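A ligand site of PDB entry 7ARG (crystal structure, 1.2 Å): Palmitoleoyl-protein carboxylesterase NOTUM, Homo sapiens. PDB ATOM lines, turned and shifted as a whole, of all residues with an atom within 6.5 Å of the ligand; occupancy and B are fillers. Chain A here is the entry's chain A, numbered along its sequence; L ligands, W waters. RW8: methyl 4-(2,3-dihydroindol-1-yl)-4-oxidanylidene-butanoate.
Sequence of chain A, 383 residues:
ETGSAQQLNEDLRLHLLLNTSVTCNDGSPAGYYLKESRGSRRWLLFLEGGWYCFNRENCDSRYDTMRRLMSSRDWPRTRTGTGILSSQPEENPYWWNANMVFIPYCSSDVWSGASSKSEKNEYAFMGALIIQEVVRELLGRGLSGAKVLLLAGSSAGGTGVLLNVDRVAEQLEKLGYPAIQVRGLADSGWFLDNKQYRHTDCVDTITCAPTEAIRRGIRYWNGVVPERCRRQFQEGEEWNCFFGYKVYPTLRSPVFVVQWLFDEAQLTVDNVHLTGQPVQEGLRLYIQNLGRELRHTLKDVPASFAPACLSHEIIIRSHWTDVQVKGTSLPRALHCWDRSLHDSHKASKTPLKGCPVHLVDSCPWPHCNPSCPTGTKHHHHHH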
ATOM      1  N   GLU A  48     -21.744 -34.951   3.785  1.00  0.00           N
ATOM      2  CA  GLU A  48     -22.426 -34.804   2.514  1.00  0.00           C
ATOM      3  C   GLU A  48     -23.471 -33.671   2.641  1.00  0.00           C
ATOM      4  O   GLU A  48     -24.002 -33.390   3.728  1.00  0.00           O
ATOM      5  CB  GLU A  48     -23.169 -36.107   2.233  1.00  0.00           C
ATOM      6  CG  GLU A  48     -23.938 -36.104   0.948  1.00  0.00           C
ATOM      7  CD  GLU A  48     -24.659 -37.389   0.663  1.00  0.00           C
ATOM      8  OE1 GLU A  48     -25.045 -38.095   1.589  1.00  0.00           O
ATOM      9  OE2 GLU A  48     -24.887 -37.713  -0.532  1.00  0.00           O
ATOM     10  N   GLY A  49     -23.774 -33.034   1.511  1.00  0.00           N
ATOM     11  CA  GLY A  49     -24.847 -32.059   1.423  1.00  0.00           C
ATOM     12  C   GLY A  49     -26.093 -32.599   0.726  1.00  0.00           C
ATOM     13  O   GLY A  49     -26.269 -33.799   0.533  1.00  0.00           O
ATOM     14  N   GLY A  50     -26.980 -31.666   0.396  1.00  0.00           N
ATOM     15  CA  GLY A  50     -28.225 -31.990  -0.282  1.00  0.00           C
ATOM     16  C   GLY A  50     -29.433 -31.238   0.244  1.00  0.00           C
ATOM     17  O   GLY A  50     -30.471 -31.872   0.513  1.00  0.00           O
ATOM     18  N   TRP A  51     -29.369 -29.925   0.385  1.00  0.00           N
ATOM     19  CA  TRP A  51     -30.486 -29.079   0.812  1.00  0.00           C
ATOM     20  C   TRP A  51     -30.969 -29.536   2.198  1.00  0.00           C
ATOM     21  O   TRP A  51     -30.131 -29.763   3.084  1.00  0.00           O
ATOM     22  CB  TRP A  51     -31.568 -28.977  -0.266  1.00  0.00           C
ATOM     23  CG  TRP A  51     -31.093 -28.276  -1.497  1.00  0.00           C
ATOM     24  CD1 TRP A  51     -30.485 -28.875  -2.579  1.00  0.00           C
ATOM     25  CD2 TRP A  51     -31.120 -26.869  -1.760  1.00  0.00           C
ATOM     26  NE1 TRP A  51     -30.151 -27.905  -3.518  1.00  0.00           N
ATOM     27  CE2 TRP A  51     -30.557 -26.680  -3.049  1.00  0.00           C
ATOM     28  CE3 TRP A  51     -31.602 -25.750  -1.060  1.00  0.00           C
ATOM     29  CZ2 TRP A  51     -30.411 -25.425  -3.613  1.00  0.00           C
ATOM     30  CZ3 TRP A  51     -31.475 -24.495  -1.630  1.00  0.00           C
ATOM     31  CH2 TRP A  51     -30.901 -24.343  -2.919  1.00  0.00           C
ATOM     32  N   TYR A  52     -32.288 -29.627   2.402  1.00  0.00           N
ATOM     33  CA  TYR A  52     -32.912 -29.792   3.719  1.00  0.00           C
ATOM     34  C   TYR A  52     -34.410 -29.864   3.465  1.00  0.00           C
ATOM     35  O   TYR A  52     -34.859 -29.607   2.355  1.00  0.00           O
ATOM     36  CB  TYR A  52     -32.590 -28.589   4.660  1.00  0.00           C
ATOM     37  CG  TYR A  52     -32.622 -27.238   3.951  1.00  0.00           C
ATOM     38  CD1 TYR A  52     -33.805 -26.597   3.617  1.00  0.00           C
ATOM     39  CD2 TYR A  52     -31.449 -26.609   3.581  1.00  0.00           C
ATOM     40  CE1 TYR A  52     -33.792 -25.361   2.940  1.00  0.00           C
ATOM     41  CE2 TYR A  52     -31.430 -25.399   2.921  1.00  0.00           C
ATOM     42  CZ  TYR A  52     -32.595 -24.788   2.598  1.00  0.00           C
ATOM     43  OH  TYR A  52     -32.552 -23.565   1.926  1.00  0.00           O
ATOM     44  N   TYR A 105     -25.570 -37.743   4.428  1.00  0.00           N
ATOM     45  CA  TYR A 105     -26.546 -36.782   4.938  1.00  0.00           C
ATOM     46  C   TYR A 105     -27.915 -37.429   4.840  1.00  0.00           C
ATOM     47  O   TYR A 105     -28.458 -37.560   3.749  1.00  0.00           O
ATOM     48  CB  TYR A 105     -26.467 -35.532   4.070  1.00  0.00           C
ATOM     49  CG  TYR A 105     -27.372 -34.384   4.434  1.00  0.00           C
ATOM     50  CD1 TYR A 105     -27.567 -33.980   5.753  1.00  0.00           C
ATOM     51  CD2 TYR A 105     -27.921 -33.625   3.422  1.00  0.00           C
ATOM     52  CE1 TYR A 105     -28.325 -32.871   6.041  1.00  0.00           C
ATOM     53  CE2 TYR A 105     -28.688 -32.517   3.707  1.00  0.00           C
ATOM     54  CZ  TYR A 105     -28.867 -32.136   5.008  1.00  0.00           C
ATOM     55  OH  TYR A 105     -29.633 -31.021   5.326  1.00  0.00           O
ATOM     56  N   VAL A 110     -29.465 -29.727   7.888  1.00  0.00           N
ATOM     57  CA  VAL A 110     -28.212 -28.971   7.732  1.00  0.00           C
ATOM     58  C   VAL A 110     -27.299 -29.408   8.906  1.00  0.00           C
ATOM     59  O   VAL A 110     -26.481 -28.632   9.419  1.00  0.00           O
ATOM     60  CB  VAL A 110     -28.450 -27.445   7.719  1.00  0.00           C
ATOM     61  CG1 VAL A 110     -27.146 -26.722   7.431  1.00  0.00           C
ATOM     62  CG2 VAL A 110     -29.593 -27.051   6.871  1.00  0.00           C
ATOM     63  N   SER A 154     -19.746 -30.280   2.062  1.00  0.00           N
ATOM     64  CA  SER A 154     -20.159 -29.469   0.906  1.00  0.00           C
ATOM     65  C   SER A 154     -21.638 -29.087   0.991  1.00  0.00           C
ATOM     66  O   SER A 154     -22.479 -29.924   1.341  1.00  0.00           O
ATOM     67  CB  SER A 154     -19.898 -30.200  -0.408  1.00  0.00           C
ATOM     68  OG  SER A 154     -18.503 -30.457  -0.602  1.00  0.00           O
ATOM     69  N   SER A 155     -21.960 -27.849   0.570  1.00  0.00           N
ATOM     70  CA  SER A 155     -23.325 -27.315   0.541  1.00  0.00           C
ATOM     71  C   SER A 155     -23.877 -27.377   1.964  1.00  0.00           C
ATOM     72  O   SER A 155     -23.272 -26.789   2.857  1.00  0.00           O
ATOM     73  CB  SER A 155     -24.149 -27.985  -0.562  1.00  0.00           C
ATOM     74  OG  SER A 155     -25.325 -27.202  -0.821  1.00  0.00           O
ATOM     75  N   ALA A 156     -25.002 -28.057   2.210  1.00  0.00           N
ATOM     76  CA  ALA A 156     -25.527 -28.161   3.581  1.00  0.00           C
ATOM     77  C   ALA A 156     -24.506 -28.807   4.502  1.00  0.00           C
ATOM     78  O   ALA A 156     -24.479 -28.506   5.710  1.00  0.00           O
ATOM     79  CB  ALA A 156     -26.848 -28.941   3.610  1.00  0.00           C
ATOM     80  N   GLY A 157     -23.628 -29.676   3.969  1.00  0.00           N
ATOM     81  CA  GLY A 157     -22.528 -30.220   4.760  1.00  0.00           C
ATOM     82  C   GLY A 157     -21.482 -29.188   5.086  1.00  0.00           C
ATOM     83  O   GLY A 157     -20.838 -29.269   6.128  1.00  0.00           O
ATOM     84  N   THR A 159     -22.163 -25.903   5.569  1.00  0.00           N
ATOM     85  CA  THR A 159     -22.764 -25.213   6.695  1.00  0.00           C
ATOM     86  C   THR A 159     -22.713 -26.078   7.953  1.00  0.00           C
ATOM     87  O   THR A 159     -22.446 -25.576   9.044  1.00  0.00           O
ATOM     88  CB  THR A 159     -24.190 -24.805   6.351  1.00  0.00           C
ATOM     89  OG1 THR A 159     -24.223 -24.176   5.044  1.00  0.00           O
ATOM     90  CG2 THR A 159     -24.748 -23.853   7.423  1.00  0.00           C
ATOM     91  N   SER A 188     -18.813 -24.478  -0.136  1.00  0.00           N
ATOM     92  CA  SER A 188     -20.126 -24.149  -0.723  1.00  0.00           C
ATOM     93  C   SER A 188     -21.212 -24.093   0.350  1.00  0.00           C
ATOM     94  O   SER A 188     -22.383 -24.404   0.057  1.00  0.00           O
ATOM     95  CB  SER A 188     -20.482 -25.131  -1.838  1.00  0.00           C
ATOM     96  OG  SER A 188     -19.421 -25.116  -2.829  1.00  0.00           O
ATOM     97  N   GLY A 189     -20.842 -23.715   1.557  1.00  0.00           N
ATOM     98  CA  GLY A 189     -21.775 -23.612   2.673  1.00  0.00           C
ATOM     99  C   GLY A 189     -21.863 -22.234   3.257  1.00  0.00           C
ATOM    100  O   GLY A 189     -22.363 -22.071   4.386  1.00  0.00           O
ATOM    101  N   PHE A 191     -23.419 -18.854   2.811  1.00  0.00           N
ATOM    102  CA  PHE A 191     -24.545 -18.242   2.140  1.00  0.00           C
ATOM    103  C   PHE A 191     -24.839 -16.857   2.682  1.00  0.00           C
ATOM    104  O   PHE A 191     -24.510 -16.545   3.819  1.00  0.00           O
ATOM    105  CB  PHE A 191     -25.798 -19.129   2.265  1.00  0.00           C
ATOM    106  CG  PHE A 191     -25.592 -20.467   1.597  1.00  0.00           C
ATOM    107  CD1 PHE A 191     -25.471 -20.511   0.225  1.00  0.00           C
ATOM    108  CD2 PHE A 191     -25.421 -21.638   2.316  1.00  0.00           C
ATOM    109  CE1 PHE A 191     -25.224 -21.735  -0.412  1.00  0.00           C
ATOM    110  CE2 PHE A 191     -25.196 -22.835   1.680  1.00  0.00           C
ATOM    111  CZ  PHE A 191     -25.105 -22.891   0.342  1.00  0.00           C
ATOM    112  N   CYS A 208     -36.958 -20.969  -1.948  1.00  0.00           N
ATOM    113  CA  CYS A 208     -37.371 -20.235  -0.754  1.00  0.00           C
ATOM    114  C   CYS A 208     -36.207 -19.377  -0.255  1.00  0.00           C
ATOM    115  O   CYS A 208     -35.042 -19.794  -0.295  1.00  0.00           O
ATOM    116  CB  CYS A 208     -37.791 -21.202   0.337  1.00  0.00           C
ATOM    117  SG  CYS A 208     -38.309 -20.412   1.885  1.00  0.00           S
ATOM    118  N   PRO A 210     -33.711 -18.268   2.304  1.00  0.00           N
ATOM    119  CA  PRO A 210     -33.168 -19.173   3.339  1.00  0.00           C
ATOM    120  C   PRO A 210     -33.441 -18.759   4.785  1.00  0.00           C
ATOM    121  O   PRO A 210     -33.567 -19.637   5.650  1.00  0.00           O
ATOM    122  CB  PRO A 210     -31.669 -19.240   2.994  1.00  0.00           C
ATOM    123  CG  PRO A 210     -31.416 -17.959   2.208  1.00  0.00           C
ATOM    124  CD  PRO A 210     -32.673 -17.692   1.435  1.00  0.00           C
ATOM    125  N   ILE A 214     -34.900 -21.705   7.283  1.00  0.00           N
ATOM    126  CA  ILE A 214     -34.110 -22.108   8.448  1.00  0.00           C
ATOM    127  C   ILE A 214     -34.812 -21.740   9.755  1.00  0.00           C
ATOM    128  O   ILE A 214     -34.791 -22.507  10.720  1.00  0.00           O
ATOM    129  CB  ILE A 214     -32.694 -21.514   8.352  1.00  0.00           C
ATOM    130  CG1 ILE A 214     -31.947 -22.166   7.187  1.00  0.00           C
ATOM    131  CG2 ILE A 214     -31.901 -21.736   9.640  1.00  0.00           C
ATOM    132  CD1 ILE A 214     -31.012 -21.227   6.542  1.00  0.00           C
ATOM    133  N   PHE A 242     -26.739 -20.011  10.962  1.00  0.00           N
ATOM    134  CA  PHE A 242     -26.601 -20.818   9.751  1.00  0.00           C
ATOM    135  C   PHE A 242     -25.947 -20.045   8.616  1.00  0.00           C
ATOM    136  O   PHE A 242     -25.714 -20.630   7.568  1.00  0.00           O
ATOM    137  CB  PHE A 242     -27.957 -21.357   9.284  1.00  0.00           C
ATOM    138  CG  PHE A 242     -28.498 -22.479  10.118  1.00  0.00           C
ATOM    139  CD1 PHE A 242     -28.828 -22.289  11.449  1.00  0.00           C
ATOM    140  CD2 PHE A 242     -28.788 -23.710   9.537  1.00  0.00           C
ATOM    141  CE1 PHE A 242     -29.401 -23.352  12.215  1.00  0.00           C
ATOM    142  CE2 PHE A 242     -29.355 -24.746  10.313  1.00  0.00           C
ATOM    143  CZ  PHE A 242     -29.628 -24.561  11.629  1.00  0.00           C
ATOM    144  N   PHE A 243     -25.655 -18.745   8.835  1.00  0.00           N
ATOM    145  CA  PHE A 243     -25.065 -17.882   7.808  1.00  0.00           C
ATOM    146  C   PHE A 243     -23.601 -17.689   8.173  1.00  0.00           C
ATOM    147  O   PHE A 243     -23.290 -17.117   9.214  1.00  0.00           O
ATOM    148  CB  PHE A 243     -25.877 -16.605   7.670  1.00  0.00           C
ATOM    149  CG  PHE A 243     -27.183 -16.905   7.020  1.00  0.00           C
ATOM    150  CD1 PHE A 243     -27.276 -16.953   5.670  1.00  0.00           C
ATOM    151  CD2 PHE A 243     -28.261 -17.315   7.804  1.00  0.00           C
ATOM    152  CE1 PHE A 243     -28.474 -17.324   5.046  1.00  0.00           C
ATOM    153  CE2 PHE A 243     -29.428 -17.692   7.217  1.00  0.00           C
ATOM    154  CZ  PHE A 243     -29.547 -17.692   5.844  1.00  0.00           C
ATOM    155  N   ASP A 263     -22.317 -18.763  -6.359  1.00  0.00           N
ATOM    156  CA  ASP A 263     -22.742 -20.141  -6.118  1.00  0.00           C
ATOM    157  C   ASP A 263     -24.135 -20.384  -6.685  1.00  0.00           C
ATOM    158  O   ASP A 263     -25.043 -19.570  -6.475  1.00  0.00           O
ATOM    159  CB  ASP A 263     -22.700 -20.390  -4.611  1.00  0.00           C
ATOM    160  CG  ASP A 263     -23.021 -21.772  -4.265  1.00  0.00           C
ATOM    161  OD1 ASP A 263     -22.133 -22.630  -4.265  1.00  0.00           O
ATOM    162  OD2 ASP A 263     -24.215 -22.018  -4.017  1.00  0.00           O
ATOM    163  N   ALA A 265     -26.466 -22.449  -5.844  1.00  0.00           N
ATOM    164  CA  ALA A 265     -27.518 -22.576  -4.846  1.00  0.00           C
ATOM    165  C   ALA A 265     -27.876 -21.216  -4.261  1.00  0.00           C
ATOM    166  O   ALA A 265     -29.051 -20.958  -3.965  1.00  0.00           O
ATOM    167  CB  ALA A 265     -27.104 -23.560  -3.756  1.00  0.00           C
ATOM    168  N   GLN A 266     -26.884 -20.337  -4.065  1.00  0.00           N
ATOM    169  CA  GLN A 266     -27.176 -18.963  -3.672  1.00  0.00           C
ATOM    170  C   GLN A 266     -28.059 -18.286  -4.713  1.00  0.00           C
ATOM    171  O   GLN A 266     -29.074 -17.664  -4.376  1.00  0.00           O
ATOM    172  CB  GLN A 266     -25.866 -18.182  -3.490  1.00  0.00           C
ATOM    173  CG  GLN A 266     -26.078 -16.720  -3.123  1.00  0.00           C
ATOM    174  CD  GLN A 266     -26.448 -16.555  -1.658  1.00  0.00           C
ATOM    175  OE1 GLN A 266     -25.772 -17.069  -0.774  1.00  0.00           O
ATOM    176  NE2 GLN A 266     -27.533 -15.821  -1.408  1.00  0.00           N
ATOM    177  N   VAL A 269     -31.748 -19.709  -4.463  1.00  0.00           N
ATOM    178  CA  VAL A 269     -32.554 -19.160  -3.377  1.00  0.00           C
ATOM    179  C   VAL A 269     -32.819 -17.693  -3.614  1.00  0.00           C
ATOM    180  O   VAL A 269     -33.816 -17.165  -3.086  1.00  0.00           O
ATOM    181  CB  VAL A 269     -31.995 -19.430  -1.964  1.00  0.00           C
ATOM    182  CG1 VAL A 269     -31.813 -20.919  -1.727  1.00  0.00           C
ATOM    183  CG2 VAL A 269     -30.664 -18.733  -1.739  1.00  0.00           C
ATOM    184  N   HIS A 312     -21.007 -24.963  -8.163  1.00  0.00           N
ATOM    185  CA  HIS A 312     -21.587 -25.453  -6.907  1.00  0.00           C
ATOM    186  C   HIS A 312     -20.854 -26.678  -6.394  1.00  0.00           C
ATOM    187  O   HIS A 312     -20.872 -27.720  -7.062  1.00  0.00           O
ATOM    188  CB  HIS A 312     -23.089 -25.736  -7.065  1.00  0.00           C
ATOM    189  CG  HIS A 312     -23.752 -26.226  -5.810  1.00  0.00           C
ATOM    190  ND1 HIS A 312     -23.830 -25.471  -4.659  1.00  0.00           N
ATOM    191  CD2 HIS A 312     -24.366 -27.401  -5.541  1.00  0.00           C
ATOM    192  CE1 HIS A 312     -24.455 -26.178  -3.733  1.00  0.00           C
ATOM    193  NE2 HIS A 312     -24.792 -27.347  -4.232  1.00  0.00           N
ATOM    194  N   GLU A 313     -20.293 -26.555  -5.185  1.00  0.00           N
ATOM    195  CA  GLU A 313     -19.445 -27.548  -4.509  1.00  0.00           C
ATOM    196  C   GLU A 313     -18.152 -27.702  -5.284  1.00  0.00           C
ATOM    197  O   GLU A 313     -18.073 -27.252  -6.429  1.00  0.00           O
ATOM    198  CB  GLU A 313     -20.134 -28.894  -4.259  1.00  0.00           C
ATOM    199  CG  GLU A 313     -21.471 -28.768  -3.612  1.00  0.00           C
ATOM    200  CD  GLU A 313     -22.170 -30.093  -3.473  1.00  0.00           C
ATOM    201  OE1 GLU A 313     -22.135 -30.880  -4.440  1.00  0.00           O
ATOM    202  OE2 GLU A 313     -22.724 -30.358  -2.388  1.00  0.00           O
HETATM  203  C03 RW8 L   1     -26.562 -27.777  -0.622  1.00  0.00           C
HETATM  204  C05 RW8 L   1     -27.661 -26.952  -1.253  1.00  0.00           C
HETATM  205  C06 RW8 L   1     -27.757 -25.496  -0.824  1.00  0.00           C
HETATM  206  C07 RW8 L   1     -27.852 -25.312   0.665  1.00  0.00           C
HETATM  207  C10 RW8 L   1     -28.652 -22.908   0.285  1.00  0.00           C
HETATM  208  C11 RW8 L   1     -29.136 -21.820   1.204  1.00  0.00           C
HETATM  209  C12 RW8 L   1     -28.719 -22.285   2.579  1.00  0.00           C
HETATM  210  C13 RW8 L   1     -28.730 -21.599   3.791  1.00  0.00           C
HETATM  211  C14 RW8 L   1     -28.264 -22.240   4.936  1.00  0.00           C
HETATM  212  C15 RW8 L   1     -27.794 -23.550   4.858  1.00  0.00           C
HETATM  213  C16 RW8 L   1     -27.769 -24.248   3.670  1.00  0.00           C
HETATM  214  C17 RW8 L   1     -28.280 -23.607   2.535  1.00  0.00           C
HETATM  215  N09 RW8 L   1     -28.281 -24.046   1.140  1.00  0.00           N
HETATM  216  O04 RW8 L   1     -26.732 -28.810  -0.098  1.00  0.00           O
HETATM  217  O08 RW8 L   1     -27.548 -26.177   1.414  1.00  0.00           O
HETATM  218  O   HOH W   1     -26.339 -29.217  -3.161  1.00  0.00           O
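The backbone NH (N) of Trp 51 is in hydrogen-bond range of an oxygen (O04) of the ligand (2.9 Å). The backbone NH (N) of Gly 50 is in hydrogen-bond range of an oxygen (O04) of the ligand (2.9 Å). C03 of the ligand is bonded to OG of Ser 155 (1.4 Å). O04 of the ligand sits at hydrogen-bond distance from N of Ala 156 (3.0 Å).
The side-chain hydroxyl (OH) of Tyr 105 sits at hydrogen-bond distance from the backbone carbonyl oxygen (O) of Trp 51 (2.6 Å). The backbone carbonyl oxygen (O) of Gly 189 is in hydrogen-bond range of the side-chain hydroxyl (OG1) of Thr 159, at 2.9 Å. The backbone NH (N) of Gly 49 sits close to the backbone carbonyl oxygen (O) of Ser 154 (3.4 Å). N of Ala 265 is in hydrogen-bond range of OD2 of Asp 263, 2.9 Å away. The side-chain hydroxyl of Ser 155 lies close to a ring nitrogen (NE2) of His 312 (3.5 Å).
C of Gly 49 touches O04 of the ligand, at 3.9 Å. Tyr 52 touches the ligand. OG1 of Thr 159 touches C15 of the ligand (3.6 Å). CE2 of Phe 191 touches C17 of the ligand, at 3.3 Å. CB of Pro 210 touches C13 of the ligand (3.9 Å). Ile 214 touches the ligand. Ala 265 touches the ligand (CB to C06, 3.6 Å). 11 residues have an atom within 4 Å of the ligand: Gly 49, Gly 50, Trp 51, Tyr 52, Ser 155, Ala 156, Thr 159, Phe 191, Pro 210, Ile 214 and Ala 265.
Water W1 lies within hydrogen-bond range of NE2 of His 312, O04 of the ligand and OG of Ser 155.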
